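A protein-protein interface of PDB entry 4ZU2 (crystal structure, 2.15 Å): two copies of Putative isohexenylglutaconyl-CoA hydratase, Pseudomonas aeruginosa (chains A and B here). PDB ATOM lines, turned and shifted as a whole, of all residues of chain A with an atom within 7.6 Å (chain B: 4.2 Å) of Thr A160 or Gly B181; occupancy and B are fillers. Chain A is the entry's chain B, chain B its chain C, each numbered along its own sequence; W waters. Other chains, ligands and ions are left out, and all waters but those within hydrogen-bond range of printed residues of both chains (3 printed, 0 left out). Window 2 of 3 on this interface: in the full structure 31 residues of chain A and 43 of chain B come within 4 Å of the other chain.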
ATOM      1  N   VAL A 154       7.452  -5.162  11.660  1.00  0.00           N
ATOM      2  CA  VAL A 154       7.324  -6.127  12.741  1.00  0.00           C
ATOM      3  C   VAL A 154       5.847  -6.419  12.947  1.00  0.00           C
ATOM      4  O   VAL A 154       5.429  -7.573  12.991  1.00  0.00           O
ATOM      5  CB  VAL A 154       7.954  -5.652  14.036  1.00  0.00           C
ATOM      6  CG1 VAL A 154       7.641  -6.639  15.173  1.00  0.00           C
ATOM      7  CG2 VAL A 154       9.463  -5.500  13.860  1.00  0.00           C
ATOM      8  N   ILE A 157       4.470  -8.589   9.615  1.00  0.00           N
ATOM      9  CA  ILE A 157       4.791  -9.984   9.411  1.00  0.00           C
ATOM     10  C   ILE A 157       5.416 -10.674  10.600  1.00  0.00           C
ATOM     11  O   ILE A 157       5.745 -11.861  10.498  1.00  0.00           O
ATOM     12  CB  ILE A 157       5.708 -10.159   8.199  1.00  0.00           C
ATOM     13  CG1 ILE A 157       7.030  -9.360   8.387  1.00  0.00           C
ATOM     14  CG2 ILE A 157       4.929  -9.817   6.929  1.00  0.00           C
ATOM     15  CD1 ILE A 157       7.843  -9.261   7.108  1.00  0.00           C
ATOM     16  N   GLY A 158       5.553  -9.975  11.728  1.00  0.00           N
ATOM     17  CA  GLY A 158       6.118 -10.595  12.910  1.00  0.00           C
ATOM     18  C   GLY A 158       7.648 -10.502  12.928  1.00  0.00           C
ATOM     19  O   GLY A 158       8.294 -10.552  11.883  1.00  0.00           O
ATOM     20  N   LEU A 159       8.223 -10.388  14.130  1.00  0.00           N
ATOM     21  CA  LEU A 159       9.671 -10.187  14.299  1.00  0.00           C
ATOM     22  C   LEU A 159      10.497 -11.244  13.574  1.00  0.00           C
ATOM     23  O   LEU A 159      11.565 -10.952  13.058  1.00  0.00           O
ATOM     24  CB  LEU A 159      10.053 -10.163  15.800  1.00  0.00           C
ATOM     25  CG  LEU A 159      11.567 -10.062  16.153  1.00  0.00           C
ATOM     26  CD1 LEU A 159      12.125  -8.660  15.974  1.00  0.00           C
ATOM     27  CD2 LEU A 159      11.847 -10.538  17.572  1.00  0.00           C
ATOM     28  N   THR A 160      10.016 -12.477  13.581  1.00  0.00           N
ATOM     29  CA  THR A 160      10.771 -13.612  13.031  1.00  0.00           C
ATOM     30  C   THR A 160      11.146 -13.407  11.545  1.00  0.00           C
ATOM     31  O   THR A 160      12.311 -13.597  11.172  1.00  0.00           O
ATOM     32  CB  THR A 160      10.030 -14.968  13.243  1.00  0.00           C
ATOM     33  OG1 THR A 160       9.777 -15.181  14.652  1.00  0.00           O
ATOM     34  CG2 THR A 160      10.902 -16.158  12.737  1.00  0.00           C
ATOM     35  N   GLN A 161      10.194 -12.986  10.707  1.00  0.00           N
ATOM     36  CA  GLN A 161      10.490 -12.710   9.293  1.00  0.00           C
ATOM     37  C   GLN A 161      11.100 -11.349   9.070  1.00  0.00           C
ATOM     38  O   GLN A 161      11.962 -11.198   8.206  1.00  0.00           O
ATOM     39  CB  GLN A 161       9.238 -12.816   8.416  1.00  0.00           C
ATOM     40  CG  GLN A 161       8.754 -14.199   8.281  1.00  0.00           C
ATOM     41  CD  GLN A 161       9.750 -15.135   7.606  1.00  0.00           C
ATOM     42  OE1 GLN A 161      10.731 -14.715   6.964  1.00  0.00           O
ATOM     43  NE2 GLN A 161       9.490 -16.425   7.745  1.00  0.00           N
ATOM     44  N   ALA A 162      10.635 -10.351   9.822  1.00  0.00           N
ATOM     45  CA  ALA A 162      11.227  -9.029   9.721  1.00  0.00           C
ATOM     46  C   ALA A 162      12.745  -9.079   9.978  1.00  0.00           C
ATOM     47  O   ALA A 162      13.491  -8.469   9.230  1.00  0.00           O
ATOM     48  CB  ALA A 162      10.591  -8.070  10.676  1.00  0.00           C
ATOM     49  N   ARG A 163      13.202  -9.789  11.014  1.00  0.00           N
ATOM     50  CA  ARG A 163      14.657  -9.761  11.342  1.00  0.00           C
ATOM     51  C   ARG A 163      15.503 -10.230  10.169  1.00  0.00           C
ATOM     52  O   ARG A 163      16.395  -9.519   9.732  1.00  0.00           O
ATOM     53  CB  ARG A 163      15.011 -10.505  12.644  1.00  0.00           C
ATOM     54  CG  ARG A 163      14.607 -11.962  12.744  1.00  0.00           C
ATOM     55  CD  ARG A 163      14.408 -12.414  14.211  1.00  0.00           C
ATOM     56  NE  ARG A 163      15.591 -12.218  15.029  1.00  0.00           N
ATOM     57  CZ  ARG A 163      15.757 -12.669  16.279  1.00  0.00           C
ATOM     58  NH1 ARG A 163      14.804 -13.328  16.925  1.00  0.00           N
ATOM     59  NH2 ARG A 163      16.895 -12.449  16.900  1.00  0.00           N
ATOM     60  N   ARG A 164      15.181 -11.388   9.618  1.00  0.00           N
ATOM     61  CA  ARG A 164      15.892 -11.917   8.481  1.00  0.00           C
ATOM     62  C   ARG A 164      15.906 -10.940   7.331  1.00  0.00           C
ATOM     63  O   ARG A 164      16.954 -10.646   6.779  1.00  0.00           O
ATOM     64  CB  ARG A 164      15.261 -13.231   8.017  1.00  0.00           C
ATOM     65  CG  ARG A 164      15.922 -13.786   6.751  1.00  0.00           C
ATOM     66  CD  ARG A 164      15.305 -15.100   6.288  1.00  0.00           C
ATOM     67  NE  ARG A 164      14.024 -14.868   5.628  1.00  0.00           N
ATOM     68  CZ  ARG A 164      13.844 -14.685   4.321  1.00  0.00           C
ATOM     69  NH1 ARG A 164      14.858 -14.715   3.472  1.00  0.00           N
ATOM     70  NH2 ARG A 164      12.620 -14.483   3.866  1.00  0.00           N
ATOM     71  N   LEU A 165      14.736 -10.451   6.958  1.00  0.00           N
ATOM     72  CA  LEU A 165      14.606  -9.616   5.766  1.00  0.00           C
ATOM     73  C   LEU A 165      15.405  -8.332   5.880  1.00  0.00           C
ATOM     74  O   LEU A 165      15.951  -7.832   4.888  1.00  0.00           O
ATOM     75  CB  LEU A 165      13.127  -9.292   5.483  1.00  0.00           C
ATOM     76  CG  LEU A 165      12.266 -10.484   5.064  1.00  0.00           C
ATOM     77  CD1 LEU A 165      10.811 -10.064   4.999  1.00  0.00           C
ATOM     78  CD2 LEU A 165      12.742 -11.070   3.691  1.00  0.00           C
ATOM     79  N   ARG A 179       2.931 -15.740   1.050  1.00  0.00           N
ATOM     80  CA  ARG A 179       3.257 -16.807   1.999  1.00  0.00           C
ATOM     81  C   ARG A 179       3.736 -16.246   3.349  1.00  0.00           C
ATOM     82  O   ARG A 179       3.506 -16.850   4.399  1.00  0.00           O
ATOM     83  CB  ARG A 179       4.343 -17.715   1.402  1.00  0.00           C
ATOM     84  CG  ARG A 179       4.812 -18.842   2.311  1.00  0.00           C
ATOM     85  CD  ARG A 179       5.969 -19.617   1.683  1.00  0.00           C
ATOM     86  NE  ARG A 179       7.265 -18.972   1.911  1.00  0.00           N
ATOM     87  CZ  ARG A 179       7.916 -19.015   3.066  1.00  0.00           C
ATOM     88  NH1 ARG A 179       7.379 -19.659   4.094  1.00  0.00           N
ATOM     89  NH2 ARG A 179       9.084 -18.407   3.209  1.00  0.00           N
ATOM     90  N   ARG B 155       6.747 -14.874  20.947  1.00  0.00           N
ATOM     91  CA  ARG B 155       7.249 -13.902  19.977  1.00  0.00           C
ATOM     92  C   ARG B 155       7.665 -14.533  18.656  1.00  0.00           C
ATOM     93  O   ARG B 155       7.669 -13.877  17.599  1.00  0.00           O
ATOM     94  CB  ARG B 155       8.488 -13.245  20.568  1.00  0.00           C
ATOM     95  CG  ARG B 155       8.603 -11.787  20.347  1.00  0.00           C
ATOM     96  CD  ARG B 155       9.187 -11.138  21.628  1.00  0.00           C
ATOM     97  NE  ARG B 155      10.118 -10.027  21.392  1.00  0.00           N
ATOM     98  CZ  ARG B 155      11.356  -9.912  21.897  1.00  0.00           C
ATOM     99  NH1 ARG B 155      11.848 -10.803  22.739  1.00  0.00           N
ATOM    100  NH2 ARG B 155      12.083  -8.853  21.587  1.00  0.00           N
ATOM    101  N   ARG B 156       8.064 -15.800  18.736  1.00  0.00           N
ATOM    102  CA  ARG B 156       8.564 -16.482  17.578  1.00  0.00           C
ATOM    103  C   ARG B 156       7.426 -16.723  16.619  1.00  0.00           C
ATOM    104  O   ARG B 156       7.481 -16.266  15.482  1.00  0.00           O
ATOM    105  CB  ARG B 156       9.224 -17.807  17.947  1.00  0.00           C
ATOM    106  CG  ARG B 156      10.014 -18.367  16.801  1.00  0.00           C
ATOM    107  CD  ARG B 156      11.271 -17.523  16.528  1.00  0.00           C
ATOM    108  NE  ARG B 156      12.146 -18.187  15.573  1.00  0.00           N
ATOM    109  CZ  ARG B 156      13.279 -17.671  15.127  1.00  0.00           C
ATOM    110  NH1 ARG B 156      13.702 -16.507  15.583  1.00  0.00           N
ATOM    111  NH2 ARG B 156      14.000 -18.331  14.237  1.00  0.00           N
ATOM    112  N   ILE B 157       6.403 -17.424  17.114  1.00  0.00           N
ATOM    113  CA  ILE B 157       5.382 -18.044  16.270  1.00  0.00           C
ATOM    114  C   ILE B 157       3.955 -17.564  16.603  1.00  0.00           C
ATOM    115  O   ILE B 157       2.990 -17.958  15.957  1.00  0.00           O
ATOM    116  CB  ILE B 157       5.438 -19.610  16.321  1.00  0.00           C
ATOM    117  CG1 ILE B 157       5.174 -20.134  17.731  1.00  0.00           C
ATOM    118  CG2 ILE B 157       6.765 -20.096  15.863  1.00  0.00           C
ATOM    119  CD1 ILE B 157       5.013 -21.670  17.857  1.00  0.00           C
ATOM    120  N   ALA B 177       7.868 -27.241  11.450  1.00  0.00           N
ATOM    121  CA  ALA B 177       8.507 -26.064  12.015  1.00  0.00           C
ATOM    122  C   ALA B 177       8.610 -24.891  11.034  1.00  0.00           C
ATOM    123  O   ALA B 177       8.710 -23.740  11.432  1.00  0.00           O
ATOM    124  CB  ALA B 177       9.860 -26.408  12.500  1.00  0.00           C
ATOM    125  N   LEU B 178       8.635 -25.183   9.751  1.00  0.00           N
ATOM    126  CA  LEU B 178       8.679 -24.131   8.740  1.00  0.00           C
ATOM    127  C   LEU B 178       7.290 -23.538   8.507  1.00  0.00           C
ATOM    128  O   LEU B 178       7.144 -22.324   8.414  1.00  0.00           O
ATOM    129  CB  LEU B 178       9.225 -24.698   7.428  1.00  0.00           C
ATOM    130  CG  LEU B 178       8.994 -23.899   6.149  1.00  0.00           C
ATOM    131  CD1 LEU B 178       9.824 -22.635   6.192  1.00  0.00           C
ATOM    132  CD2 LEU B 178       9.278 -24.718   4.899  1.00  0.00           C
ATOM    133  N   ARG B 179       6.291 -24.411   8.370  1.00  0.00           N
ATOM    134  CA  ARG B 179       4.902 -23.997   8.216  1.00  0.00           C
ATOM    135  C   ARG B 179       4.449 -23.125   9.402  1.00  0.00           C
ATOM    136  O   ARG B 179       3.683 -22.162   9.210  1.00  0.00           O
ATOM    137  CB  ARG B 179       3.998 -25.224   8.114  1.00  0.00           C
ATOM    138  CG  ARG B 179       2.519 -24.926   7.771  1.00  0.00           C
ATOM    139  CD  ARG B 179       1.603 -26.149   8.036  1.00  0.00           C
ATOM    140  NE  ARG B 179       1.538 -26.532   9.459  1.00  0.00           N
ATOM    141  CZ  ARG B 179       0.559 -26.203  10.305  1.00  0.00           C
ATOM    142  NH1 ARG B 179      -0.488 -25.476   9.908  1.00  0.00           N
ATOM    143  NH2 ARG B 179       0.612 -26.604  11.568  1.00  0.00           N
ATOM    144  N   LEU B 180       4.914 -23.482  10.610  1.00  0.00           N
ATOM    145  CA  LEU B 180       4.593 -22.763  11.855  1.00  0.00           C
ATOM    146  C   LEU B 180       5.367 -21.461  12.000  1.00  0.00           C
ATOM    147  O   LEU B 180       5.149 -20.707  12.938  1.00  0.00           O
ATOM    148  CB  LEU B 180       4.892 -23.617  13.103  1.00  0.00           C
ATOM    149  CG  LEU B 180       4.079 -24.884  13.402  1.00  0.00           C
ATOM    150  CD1 LEU B 180       4.496 -25.474  14.729  1.00  0.00           C
ATOM    151  CD2 LEU B 180       2.582 -24.612  13.421  1.00  0.00           C
ATOM    152  N   GLY B 181       6.295 -21.211  11.086  1.00  0.00           N
ATOM    153  CA  GLY B 181       7.100 -20.007  11.138  1.00  0.00           C
ATOM    154  C   GLY B 181       8.219 -20.067  12.179  1.00  0.00           C
ATOM    155  O   GLY B 181       8.797 -19.045  12.522  1.00  0.00           O
ATOM    156  N   LEU B 182       8.522 -21.255  12.689  1.00  0.00           N
ATOM    157  CA  LEU B 182       9.555 -21.397  13.702  1.00  0.00           C
ATOM    158  C   LEU B 182      10.947 -21.201  13.127  1.00  0.00           C
ATOM    159  O   LEU B 182      11.800 -20.628  13.782  1.00  0.00           O
ATOM    160  CB  LEU B 182       9.468 -22.759  14.379  1.00  0.00           C
ATOM    161  CG  LEU B 182      10.326 -22.976  15.622  1.00  0.00           C
ATOM    162  CD1 LEU B 182       9.893 -22.044  16.697  1.00  0.00           C
ATOM    163  CD2 LEU B 182      10.178 -24.398  16.109  1.00  0.00           C
ATOM    164  N   VAL B 183      11.158 -21.684  11.908  1.00  0.00           N
ATOM    165  CA  VAL B 183      12.424 -21.523  11.212  1.00  0.00           C
ATOM    166  C   VAL B 183      12.088 -20.979   9.836  1.00  0.00           C
ATOM    167  O   VAL B 183      10.915 -20.901   9.463  1.00  0.00           O
ATOM    168  CB  VAL B 183      13.215 -22.846  11.123  1.00  0.00           C
ATOM    169  CG1 VAL B 183      13.296 -23.490  12.480  1.00  0.00           C
ATOM    170  CG2 VAL B 183      12.593 -23.806  10.121  1.00  0.00           C
ATOM    171  N   HIS B 184      13.102 -20.570   9.097  1.00  0.00           N
ATOM    172  CA  HIS B 184      12.883 -19.812   7.885  1.00  0.00           C
ATOM    173  C   HIS B 184      13.044 -20.694   6.682  1.00  0.00           C
ATOM    174  O   HIS B 184      12.459 -20.436   5.635  1.00  0.00           O
ATOM    175  CB  HIS B 184      13.872 -18.655   7.811  1.00  0.00           C
ATOM    176  CG  HIS B 184      13.769 -17.717   8.961  1.00  0.00           C
ATOM    177  ND1 HIS B 184      14.375 -17.969  10.171  1.00  0.00           N
ATOM    178  CD2 HIS B 184      13.104 -16.546   9.110  1.00  0.00           C
ATOM    179  CE1 HIS B 184      14.099 -16.989  11.015  1.00  0.00           C
ATOM    180  NE2 HIS B 184      13.340 -16.104  10.389  1.00  0.00           N
HETATM  181  O   HOH W   1       8.861 -19.638   8.082  1.00  0.00           O
HETATM  182  O   HOH W   2      11.698 -14.118  16.490  1.00  0.00           O
HETATM  183  O   HOH W   3       7.229 -13.120  15.008  1.00  0.00           O
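Positions printed for both chains: 157 and 179.
Thr A160 touches Arg B155 (OG1 to O, 3.9 Å).
Gly B181 touches Thr A160 (O to CG2, 3.6 Å).
OE1 of Gln A161 touches CD2 of His B184 (3.7 Å).
Arg A163 touches Arg B156 (NH1 to NH1, 3.6 Å).
Arg A164 touches His B184.
The side-chain hydroxyl (OG1) of Thr A160 is in hydrogen-bond range of the backbone carbonyl oxygen (O) of Arg B156, at 2.7 Å.
NE2 of His B184 is in hydrogen-bond range of O of Thr A160.
Printed residues of chain A that touch a printed residue of chain B: Thr A160, Gln A161, Arg A163 and Arg A164.
Along chain A the printed residues that touch a printed residue of chain B span positions 160 to 164.
Of the 11 printed residues of chain B, 4 touch a printed residue of chain A.
Hydrophobic or aromatic side chains of chain B that line the printed part of chain A: His B184.
Along chain B the printed residues that touch a printed residue of chain A span positions 155 to 184.
Among the printed residues, 7 pairs touch across the chains.
Among the printed residues, no Asp or Glu carboxylate lies within 4 Å of a Lys or Arg side-chain nitrogen of the other chain.
Water W3 lies within hydrogen-bond range of O of Arg B155, N of Leu A159, O of Arg B156 and N of Thr A160.
Water W1 lies within hydrogen-bond range of O of Val B183 (2.8 Å), O of Leu B178 (3.2 Å) and NE2 of Gln A161 (3.3 Å).
Water W2 lies within hydrogen-bond range of the side-chain hydroxyl (OG1) of Thr A160 (2.9 Å), the guanidinium group (NH1) of Arg A163 (3.2 Å) and the guanidinium group (NH1) of Arg B156 (3.2 Å).
The guanidinium group (NE) of Arg B156 lies within hydrogen-bond range of the backbone carbonyl oxygen (O) of Leu B182, at 3.0 Å.
Thr A160 touches just these residues of chain B: Arg B155, Arg B156, Gly B181 and His B184.
Of chain A, only Thr A160 (3.6 Å) comes within 4 Å of Gly B181.
Of the printed residues of chain A, His B184 touches Thr A160, Gln A161 and Arg A164.
Printed residues of chain A within 4 Å of Arg B156: Thr A160 (2.7 Å) and Arg A163 (3.6 Å).
Of the printed residues of chain A, Arg B155 touches Thr A160 (3.9 Å).
Arg A179 touches none of the printed residues of chain B.
Arg B179 touches none of the printed residues of chain A.
The nearest printed residue of chain B that does not touch Thr A160 is Leu B182 (4.7 Å).
The nearest residue of chain A that does not touch Gly B181 is Gln A161 (5.5 Å).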
